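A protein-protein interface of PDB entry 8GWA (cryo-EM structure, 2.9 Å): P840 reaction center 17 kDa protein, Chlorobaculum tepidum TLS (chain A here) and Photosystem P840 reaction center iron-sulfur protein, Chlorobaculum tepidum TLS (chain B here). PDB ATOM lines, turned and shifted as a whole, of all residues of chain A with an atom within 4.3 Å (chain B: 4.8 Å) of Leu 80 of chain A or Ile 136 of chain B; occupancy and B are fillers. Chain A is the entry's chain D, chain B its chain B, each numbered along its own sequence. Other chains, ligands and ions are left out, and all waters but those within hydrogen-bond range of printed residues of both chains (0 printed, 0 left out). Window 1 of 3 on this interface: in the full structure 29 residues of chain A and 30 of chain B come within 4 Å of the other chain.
Tyr 78 of chain A touches none of the printed residues of chain B. Printed residues of chain B within 4 Å of Leu 80 of chain A: Ile 136 (3.6 Å), Ile 197 (3.8 Å) and Val 205 (3.5 Å). Of the printed residues of chain B, Thr 82 of chain A touches Phe 134 (3.5 Å). Printed residues of chain A within 4 Å of Ile 136 of chain B: Leu 80 (3.6 Å), Met 114 (3.4 Å), Arg 115 (3.998 Å) and Glu 116 (3.2 Å). Printed residues of chain A within 4 Å of Asn 138 of chain B: Arg 115 (2.2 Å) and Glu 116 (3.5 Å). Of the printed residues of chain A, Leu 139 of chain B touches Glu 116 (3.1 Å). The nearest residue of chain B that does not touch Leu 80 of chain A is Val 199 of chain B (4.6 Å). The nearest printed residue of chain A that does not touch Ile 136 of chain B is Phe 35 of chain A (4.3 Å). The nearest printed residue of chain A that does not touch Ile 135 of chain B is Arg 115 of chain A (5.2 Å).
Hydrophobic or aromatic side chains of chain B within 4 Å of the printed part of chain A: Phe 134, Ile 136, Leu 139, Ile 197 and Val 205. Hydrophobic or aromatic side chains of chain A within 4 Å of the printed part of chain B: Phe 35, Leu 80 and Met 114. Among the printed residues, no Asp or Glu carboxylate lies within 4 Å of a Lys or Arg side-chain nitrogen of the other chain.
O of Arg 115 of chain A sits at hydrogen-bond distance from N of Thr 81 of chain A, at 3.1 Å. The backbone NH (N) of Ile 136 of chain B sits at hydrogen-bond distance from the backbone carbonyl oxygen (O) of Ala 195 of chain B (3.1 Å).
Among the printed residues, pairs that only touch across the chains: Phe 35 of chain A with Val 205 of chain B, Leu 80 of chain A with Ile 136 of chain B, Leu 80 of chain A with Ile 197 of chain B, Leu 80 of chain A with Val 205 of chain B, Thr 82 of chain A with Phe 134 of chain B, Met 114 of chain A with Phe 134 of chain B, Met 114 of chain A with Ile 136 of chain B, Met 114 of chain A with Ile 197 of chain B, Arg 115 of chain A with Ile 136 of chain B, Glu 116 of chain A with Ile 136 of chain B, Glu 116 of chain A with Asn 138 of chain B and Glu 116 of chain A with Leu 139 of chain B.
N of Glu 137 of chain B is in hydrogen-bond range of O of Met 114 of chain A (2.6 Å). The backbone carbonyl oxygen (O) of Glu 137 of chain B lies within hydrogen-bond range of the guanidinium group (NE) of Arg 115 of chain A. The guanidinium group (NE) of Arg 115 of chain A sits close to the side-chain amide oxygen (OD1) of Asn 138 of chain B (3.1 Å). O of Ile 135 of chain B sits close to O of Met 114 of chain A (3.2 Å).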
ATOM      1  N   PHE A  35      18.608 -14.175  -2.698  1.00  0.00           N
ATOM      2  CA  PHE A  35      19.503 -14.442  -1.585  1.00  0.00           C
ATOM      3  C   PHE A  35      18.929 -15.544  -0.706  1.00  0.00           C
ATOM      4  O   PHE A  35      17.743 -15.520  -0.365  1.00  0.00           O
ATOM      5  CB  PHE A  35      19.726 -13.182  -0.747  1.00  0.00           C
ATOM      6  CG  PHE A  35      20.683 -12.206  -1.360  1.00  0.00           C
ATOM      7  CD1 PHE A  35      22.023 -12.521  -1.497  1.00  0.00           C
ATOM      8  CD2 PHE A  35      20.246 -10.965  -1.786  1.00  0.00           C
ATOM      9  CE1 PHE A  35      22.904 -11.621  -2.054  1.00  0.00           C
ATOM     10  CE2 PHE A  35      21.123 -10.062  -2.343  1.00  0.00           C
ATOM     11  CZ  PHE A  35      22.454 -10.390  -2.473  1.00  0.00           C
ATOM     12  N   TYR A  78      22.391 -16.370  -4.288  1.00  0.00           N
ATOM     13  CA  TYR A  78      23.591 -16.183  -3.486  1.00  0.00           C
ATOM     14  C   TYR A  78      23.251 -16.412  -2.018  1.00  0.00           C
ATOM     15  O   TYR A  78      22.083 -16.452  -1.626  1.00  0.00           O
ATOM     16  CB  TYR A  78      24.199 -14.792  -3.705  1.00  0.00           C
ATOM     17  CG  TYR A  78      24.626 -14.552  -5.134  1.00  0.00           C
ATOM     18  CD1 TYR A  78      23.704 -14.174  -6.101  1.00  0.00           C
ATOM     19  CD2 TYR A  78      25.944 -14.736  -5.526  1.00  0.00           C
ATOM     20  CE1 TYR A  78      24.086 -13.965  -7.410  1.00  0.00           C
ATOM     21  CE2 TYR A  78      26.336 -14.529  -6.834  1.00  0.00           C
ATOM     22  CZ  TYR A  78      25.403 -14.144  -7.772  1.00  0.00           C
ATOM     23  OH  TYR A  78      25.789 -13.937  -9.075  1.00  0.00           O
ATOM     24  N   ILE A  79      24.292 -16.568  -1.198  1.00  0.00           N
ATOM     25  CA  ILE A  79      24.123 -17.056   0.160  1.00  0.00           C
ATOM     26  C   ILE A  79      24.511 -16.030   1.225  1.00  0.00           C
ATOM     27  O   ILE A  79      23.921 -16.041   2.312  1.00  0.00           O
ATOM     28  CB  ILE A  79      24.903 -18.375   0.349  1.00  0.00           C
ATOM     29  CG1 ILE A  79      24.142 -19.514  -0.325  1.00  0.00           C
ATOM     30  CG2 ILE A  79      25.138 -18.698   1.817  1.00  0.00           C
ATOM     31  CD1 ILE A  79      24.746 -20.872  -0.112  1.00  0.00           C
ATOM     32  N   LEU A  80      25.440 -15.113   0.937  1.00  0.00           N
ATOM     33  CA  LEU A  80      25.858 -14.096   1.906  1.00  0.00           C
ATOM     34  C   LEU A  80      26.448 -14.747   3.161  1.00  0.00           C
ATOM     35  O   LEU A  80      25.830 -14.788   4.227  1.00  0.00           O
ATOM     36  CB  LEU A  80      24.703 -13.159   2.276  1.00  0.00           C
ATOM     37  CG  LEU A  80      24.278 -12.111   1.255  1.00  0.00           C
ATOM     38  CD1 LEU A  80      22.943 -11.542   1.664  1.00  0.00           C
ATOM     39  CD2 LEU A  80      25.318 -11.018   1.146  1.00  0.00           C
ATOM     40  N   THR A  81      27.669 -15.262   2.991  1.00  0.00           N
ATOM     41  CA  THR A  81      28.346 -16.126   3.958  1.00  0.00           C
ATOM     42  C   THR A  81      28.172 -15.692   5.410  1.00  0.00           C
ATOM     43  O   THR A  81      28.235 -16.533   6.313  1.00  0.00           O
ATOM     44  CB  THR A  81      29.841 -16.207   3.638  1.00  0.00           C
ATOM     45  OG1 THR A  81      30.464 -14.950   3.928  1.00  0.00           O
ATOM     46  CG2 THR A  81      30.060 -16.557   2.176  1.00  0.00           C
ATOM     47  N   THR A  82      27.958 -14.397   5.660  1.00  0.00           N
ATOM     48  CA  THR A  82      27.582 -13.974   7.016  1.00  0.00           C
ATOM     49  C   THR A  82      26.224 -14.529   7.466  1.00  0.00           C
ATOM     50  O   THR A  82      25.775 -14.154   8.558  1.00  0.00           O
ATOM     51  CB  THR A  82      27.544 -12.450   7.124  1.00  0.00           C
ATOM     52  OG1 THR A  82      27.379 -12.074   8.497  1.00  0.00           O
ATOM     53  CG2 THR A  82      26.376 -11.899   6.324  1.00  0.00           C
ATOM     54  N   GLN A  83      25.590 -15.375   6.660  1.00  0.00           N
ATOM     55  CA  GLN A  83      24.299 -15.945   7.015  1.00  0.00           C
ATOM     56  C   GLN A  83      24.400 -16.692   8.341  1.00  0.00           C
ATOM     57  O   GLN A  83      25.328 -17.492   8.528  1.00  0.00           O
ATOM     58  CB  GLN A  83      23.825 -16.884   5.907  1.00  0.00           C
ATOM     59  CG  GLN A  83      22.749 -17.869   6.324  1.00  0.00           C
ATOM     60  CD  GLN A  83      21.354 -17.304   6.175  1.00  0.00           C
ATOM     61  OE1 GLN A  83      21.062 -16.594   5.217  1.00  0.00           O
ATOM     62  NE2 GLN A  83      20.479 -17.626   7.121  1.00  0.00           N
ATOM     63  N   MET A 114      32.901  -9.847   4.365  1.00  0.00           N
ATOM     64  CA  MET A 114      31.772 -10.698   4.035  1.00  0.00           C
ATOM     65  C   MET A 114      31.566 -10.664   2.534  1.00  0.00           C
ATOM     66  O   MET A 114      31.675  -9.602   1.912  1.00  0.00           O
ATOM     67  CB  MET A 114      30.495 -10.240   4.734  1.00  0.00           C
ATOM     68  CG  MET A 114      29.293 -11.100   4.397  1.00  0.00           C
ATOM     69  SD  MET A 114      28.348 -10.466   3.000  1.00  0.00           S
ATOM     70  CE  MET A 114      27.187  -9.410   3.841  1.00  0.00           C
ATOM     71  N   ARG A 115      31.236 -11.816   1.958  1.00  0.00           N
ATOM     72  CA  ARG A 115      31.112 -11.924   0.516  1.00  0.00           C
ATOM     73  C   ARG A 115      29.965 -12.867   0.193  1.00  0.00           C
ATOM     74  O   ARG A 115      29.495 -13.624   1.046  1.00  0.00           O
ATOM     75  CB  ARG A 115      32.419 -12.418  -0.112  1.00  0.00           C
ATOM     76  CG  ARG A 115      33.544 -11.416   0.050  1.00  0.00           C
ATOM     77  CD  ARG A 115      34.845 -11.884  -0.543  1.00  0.00           C
ATOM     78  NE  ARG A 115      34.733 -11.978  -1.989  1.00  0.00           N
ATOM     79  CZ  ARG A 115      35.656 -12.505  -2.775  1.00  0.00           C
ATOM     80  NH1 ARG A 115      36.790 -12.970  -2.292  1.00  0.00           N
ATOM     81  NH2 ARG A 115      35.444 -12.546  -4.083  1.00  0.00           N
ATOM     82  N   GLU A 116      29.507 -12.817  -1.053  1.00  0.00           N
ATOM     83  CA  GLU A 116      28.451 -13.697  -1.528  1.00  0.00           C
ATOM     84  C   GLU A 116      29.063 -14.864  -2.290  1.00  0.00           C
ATOM     85  O   GLU A 116      30.086 -14.713  -2.964  1.00  0.00           O
ATOM     86  CB  GLU A 116      27.453 -12.959  -2.428  1.00  0.00           C
ATOM     87  CG  GLU A 116      28.014 -12.536  -3.773  1.00  0.00           C
ATOM     88  CD  GLU A 116      27.152 -11.511  -4.481  1.00  0.00           C
ATOM     89  OE1 GLU A 116      26.510 -10.686  -3.801  1.00  0.00           O
ATOM     90  OE2 GLU A 116      27.109 -11.544  -5.730  1.00  0.00           O
ATOM     91  N   PHE B 134      25.912  -4.196   6.298  1.00  0.00           N
ATOM     92  CA  PHE B 134      26.927  -5.029   5.657  1.00  0.00           C
ATOM     93  C   PHE B 134      27.452  -4.459   4.340  1.00  0.00           C
ATOM     94  O   PHE B 134      26.830  -3.585   3.729  1.00  0.00           O
ATOM     95  CB  PHE B 134      26.381  -6.440   5.408  1.00  0.00           C
ATOM     96  CG  PHE B 134      26.130  -7.230   6.661  1.00  0.00           C
ATOM     97  CD1 PHE B 134      27.170  -7.876   7.304  1.00  0.00           C
ATOM     98  CD2 PHE B 134      24.856  -7.334   7.190  1.00  0.00           C
ATOM     99  CE1 PHE B 134      26.944  -8.604   8.456  1.00  0.00           C
ATOM    100  CE2 PHE B 134      24.627  -8.061   8.340  1.00  0.00           C
ATOM    101  CZ  PHE B 134      25.672  -8.697   8.974  1.00  0.00           C
ATOM    102  N   ILE B 135      28.615  -4.944   3.912  1.00  0.00           N
ATOM    103  CA  ILE B 135      29.144  -4.690   2.577  1.00  0.00           C
ATOM    104  C   ILE B 135      29.648  -6.006   2.011  1.00  0.00           C
ATOM    105  O   ILE B 135      30.450  -6.697   2.650  1.00  0.00           O
ATOM    106  CB  ILE B 135      30.272  -3.641   2.580  1.00  0.00           C
ATOM    107  CG1 ILE B 135      29.704  -2.237   2.772  1.00  0.00           C
ATOM    108  CG2 ILE B 135      31.074  -3.717   1.289  1.00  0.00           C
ATOM    109  CD1 ILE B 135      30.763  -1.161   2.821  1.00  0.00           C
ATOM    110  N   ILE B 136      29.183  -6.349   0.814  1.00  0.00           N
ATOM    111  CA  ILE B 136      29.650  -7.542   0.119  1.00  0.00           C
ATOM    112  C   ILE B 136      31.005  -7.215  -0.495  1.00  0.00           C
ATOM    113  O   ILE B 136      31.096  -6.371  -1.389  1.00  0.00           O
ATOM    114  CB  ILE B 136      28.658  -7.990  -0.958  1.00  0.00           C
ATOM    115  CG1 ILE B 136      27.298  -8.307  -0.345  1.00  0.00           C
ATOM    116  CG2 ILE B 136      29.189  -9.203  -1.694  1.00  0.00           C
ATOM    117  CD1 ILE B 136      26.227  -8.569  -1.379  1.00  0.00           C
ATOM    118  N   GLU B 137      32.064  -7.880  -0.030  1.00  0.00           N
ATOM    119  CA  GLU B 137      33.348  -7.686  -0.692  1.00  0.00           C
ATOM    120  C   GLU B 137      33.436  -8.574  -1.925  1.00  0.00           C
ATOM    121  O   GLU B 137      34.468  -9.207  -2.169  1.00  0.00           O
ATOM    122  CB  GLU B 137      34.509  -7.995   0.258  1.00  0.00           C
ATOM    123  CG  GLU B 137      34.995  -6.821   1.087  1.00  0.00           C
ATOM    124  CD  GLU B 137      34.342  -6.749   2.447  1.00  0.00           C
ATOM    125  OE1 GLU B 137      33.261  -7.347   2.629  1.00  0.00           O
ATOM    126  OE2 GLU B 137      34.928  -6.110   3.342  1.00  0.00           O
ATOM    127  N   ASN B 138      32.371  -8.585  -2.727  1.00  0.00           N
ATOM    128  CA  ASN B 138      32.346  -9.234  -4.035  1.00  0.00           C
ATOM    129  C   ASN B 138      31.743  -8.358  -5.121  1.00  0.00           C
ATOM    130  O   ASN B 138      32.109  -8.516  -6.288  1.00  0.00           O
ATOM    131  CB  ASN B 138      31.571 -10.562  -3.975  1.00  0.00           C
ATOM    132  CG  ASN B 138      32.253 -11.673  -4.755  1.00  0.00           C
ATOM    133  OD1 ASN B 138      33.478 -11.757  -4.792  1.00  0.00           O
ATOM    134  ND2 ASN B 138      31.460 -12.543  -5.370  1.00  0.00           N
ATOM    135  N   LEU B 139      30.835  -7.442  -4.796  1.00  0.00           N
ATOM    136  CA  LEU B 139      30.424  -6.416  -5.738  1.00  0.00           C
ATOM    137  C   LEU B 139      31.116  -5.088  -5.493  1.00  0.00           C
ATOM    138  O   LEU B 139      31.292  -4.319  -6.443  1.00  0.00           O
ATOM    139  CB  LEU B 139      28.904  -6.201  -5.689  1.00  0.00           C
ATOM    140  CG  LEU B 139      28.021  -7.155  -6.500  1.00  0.00           C
ATOM    141  CD1 LEU B 139      28.298  -7.021  -8.001  1.00  0.00           C
ATOM    142  CD2 LEU B 139      28.153  -8.591  -6.040  1.00  0.00           C
ATOM    143  N   CYS B 140      31.549  -4.829  -4.262  1.00  0.00           N
ATOM    144  CA  CYS B 140      32.085  -3.525  -3.905  1.00  0.00           C
ATOM    145  C   CYS B 140      33.314  -3.190  -4.735  1.00  0.00           C
ATOM    146  O   CYS B 140      34.228  -4.005  -4.886  1.00  0.00           O
ATOM    147  CB  CYS B 140      32.435  -3.493  -2.419  1.00  0.00           C
ATOM    148  SG  CYS B 140      33.351  -2.031  -1.908  1.00  0.00           S
ATOM    149  N   GLY B 194      25.768  -2.393  -5.936  1.00  0.00           N
ATOM    150  CA  GLY B 194      24.865  -3.157  -5.096  1.00  0.00           C
ATOM    151  C   GLY B 194      25.562  -4.024  -4.072  1.00  0.00           C
ATOM    152  O   GLY B 194      25.147  -5.167  -3.842  1.00  0.00           O
ATOM    153  N   ALA B 195      26.622  -3.509  -3.451  1.00  0.00           N
ATOM    154  CA  ALA B 195      27.308  -4.241  -2.396  1.00  0.00           C
ATOM    155  C   ALA B 195      26.660  -4.015  -1.037  1.00  0.00           C
ATOM    156  O   ALA B 195      26.591  -4.941  -0.223  1.00  0.00           O
ATOM    157  CB  ALA B 195      28.783  -3.843  -2.347  1.00  0.00           C
ATOM    158  N   ILE B 197      23.576  -3.944   1.297  1.00  0.00           N
ATOM    159  CA  ILE B 197      22.424  -4.828   1.217  1.00  0.00           C
ATOM    160  C   ILE B 197      21.335  -4.466   2.221  1.00  0.00           C
ATOM    161  O   ILE B 197      20.154  -4.441   1.864  1.00  0.00           O
ATOM    162  CB  ILE B 197      22.844  -6.307   1.365  1.00  0.00           C
ATOM    163  CG1 ILE B 197      23.765  -6.500   2.566  1.00  0.00           C
ATOM    164  CG2 ILE B 197      23.505  -6.793   0.090  1.00  0.00           C
ATOM    165  CD1 ILE B 197      24.016  -7.945   2.912  1.00  0.00           C
ATOM    166  N   VAL B 199      20.369  -6.220   5.239  1.00  0.00           N
ATOM    167  CA  VAL B 199      19.547  -7.358   5.630  1.00  0.00           C
ATOM    168  C   VAL B 199      18.501  -6.889   6.633  1.00  0.00           C
ATOM    169  O   VAL B 199      18.809  -6.182   7.601  1.00  0.00           O
ATOM    170  CB  VAL B 199      20.418  -8.497   6.186  1.00  0.00           C
ATOM    171  CG1 VAL B 199      21.401  -8.967   5.133  1.00  0.00           C
ATOM    172  CG2 VAL B 199      21.165  -8.063   7.439  1.00  0.00           C
ATOM    173  N   VAL B 205      16.912  -9.583   2.610  1.00  0.00           N
ATOM    174  CA  VAL B 205      18.104  -8.890   2.137  1.00  0.00           C
ATOM    175  C   VAL B 205      17.695  -7.952   1.014  1.00  0.00           C
ATOM    176  O   VAL B 205      17.265  -8.403  -0.055  1.00  0.00           O
ATOM    177  CB  VAL B 205      19.184  -9.869   1.660  1.00  0.00           C
ATOM    178  CG1 VAL B 205      20.433  -9.104   1.268  1.00  0.00           C
ATOM    179  CG2 VAL B 205      19.486 -10.894   2.741  1.00  0.00           C
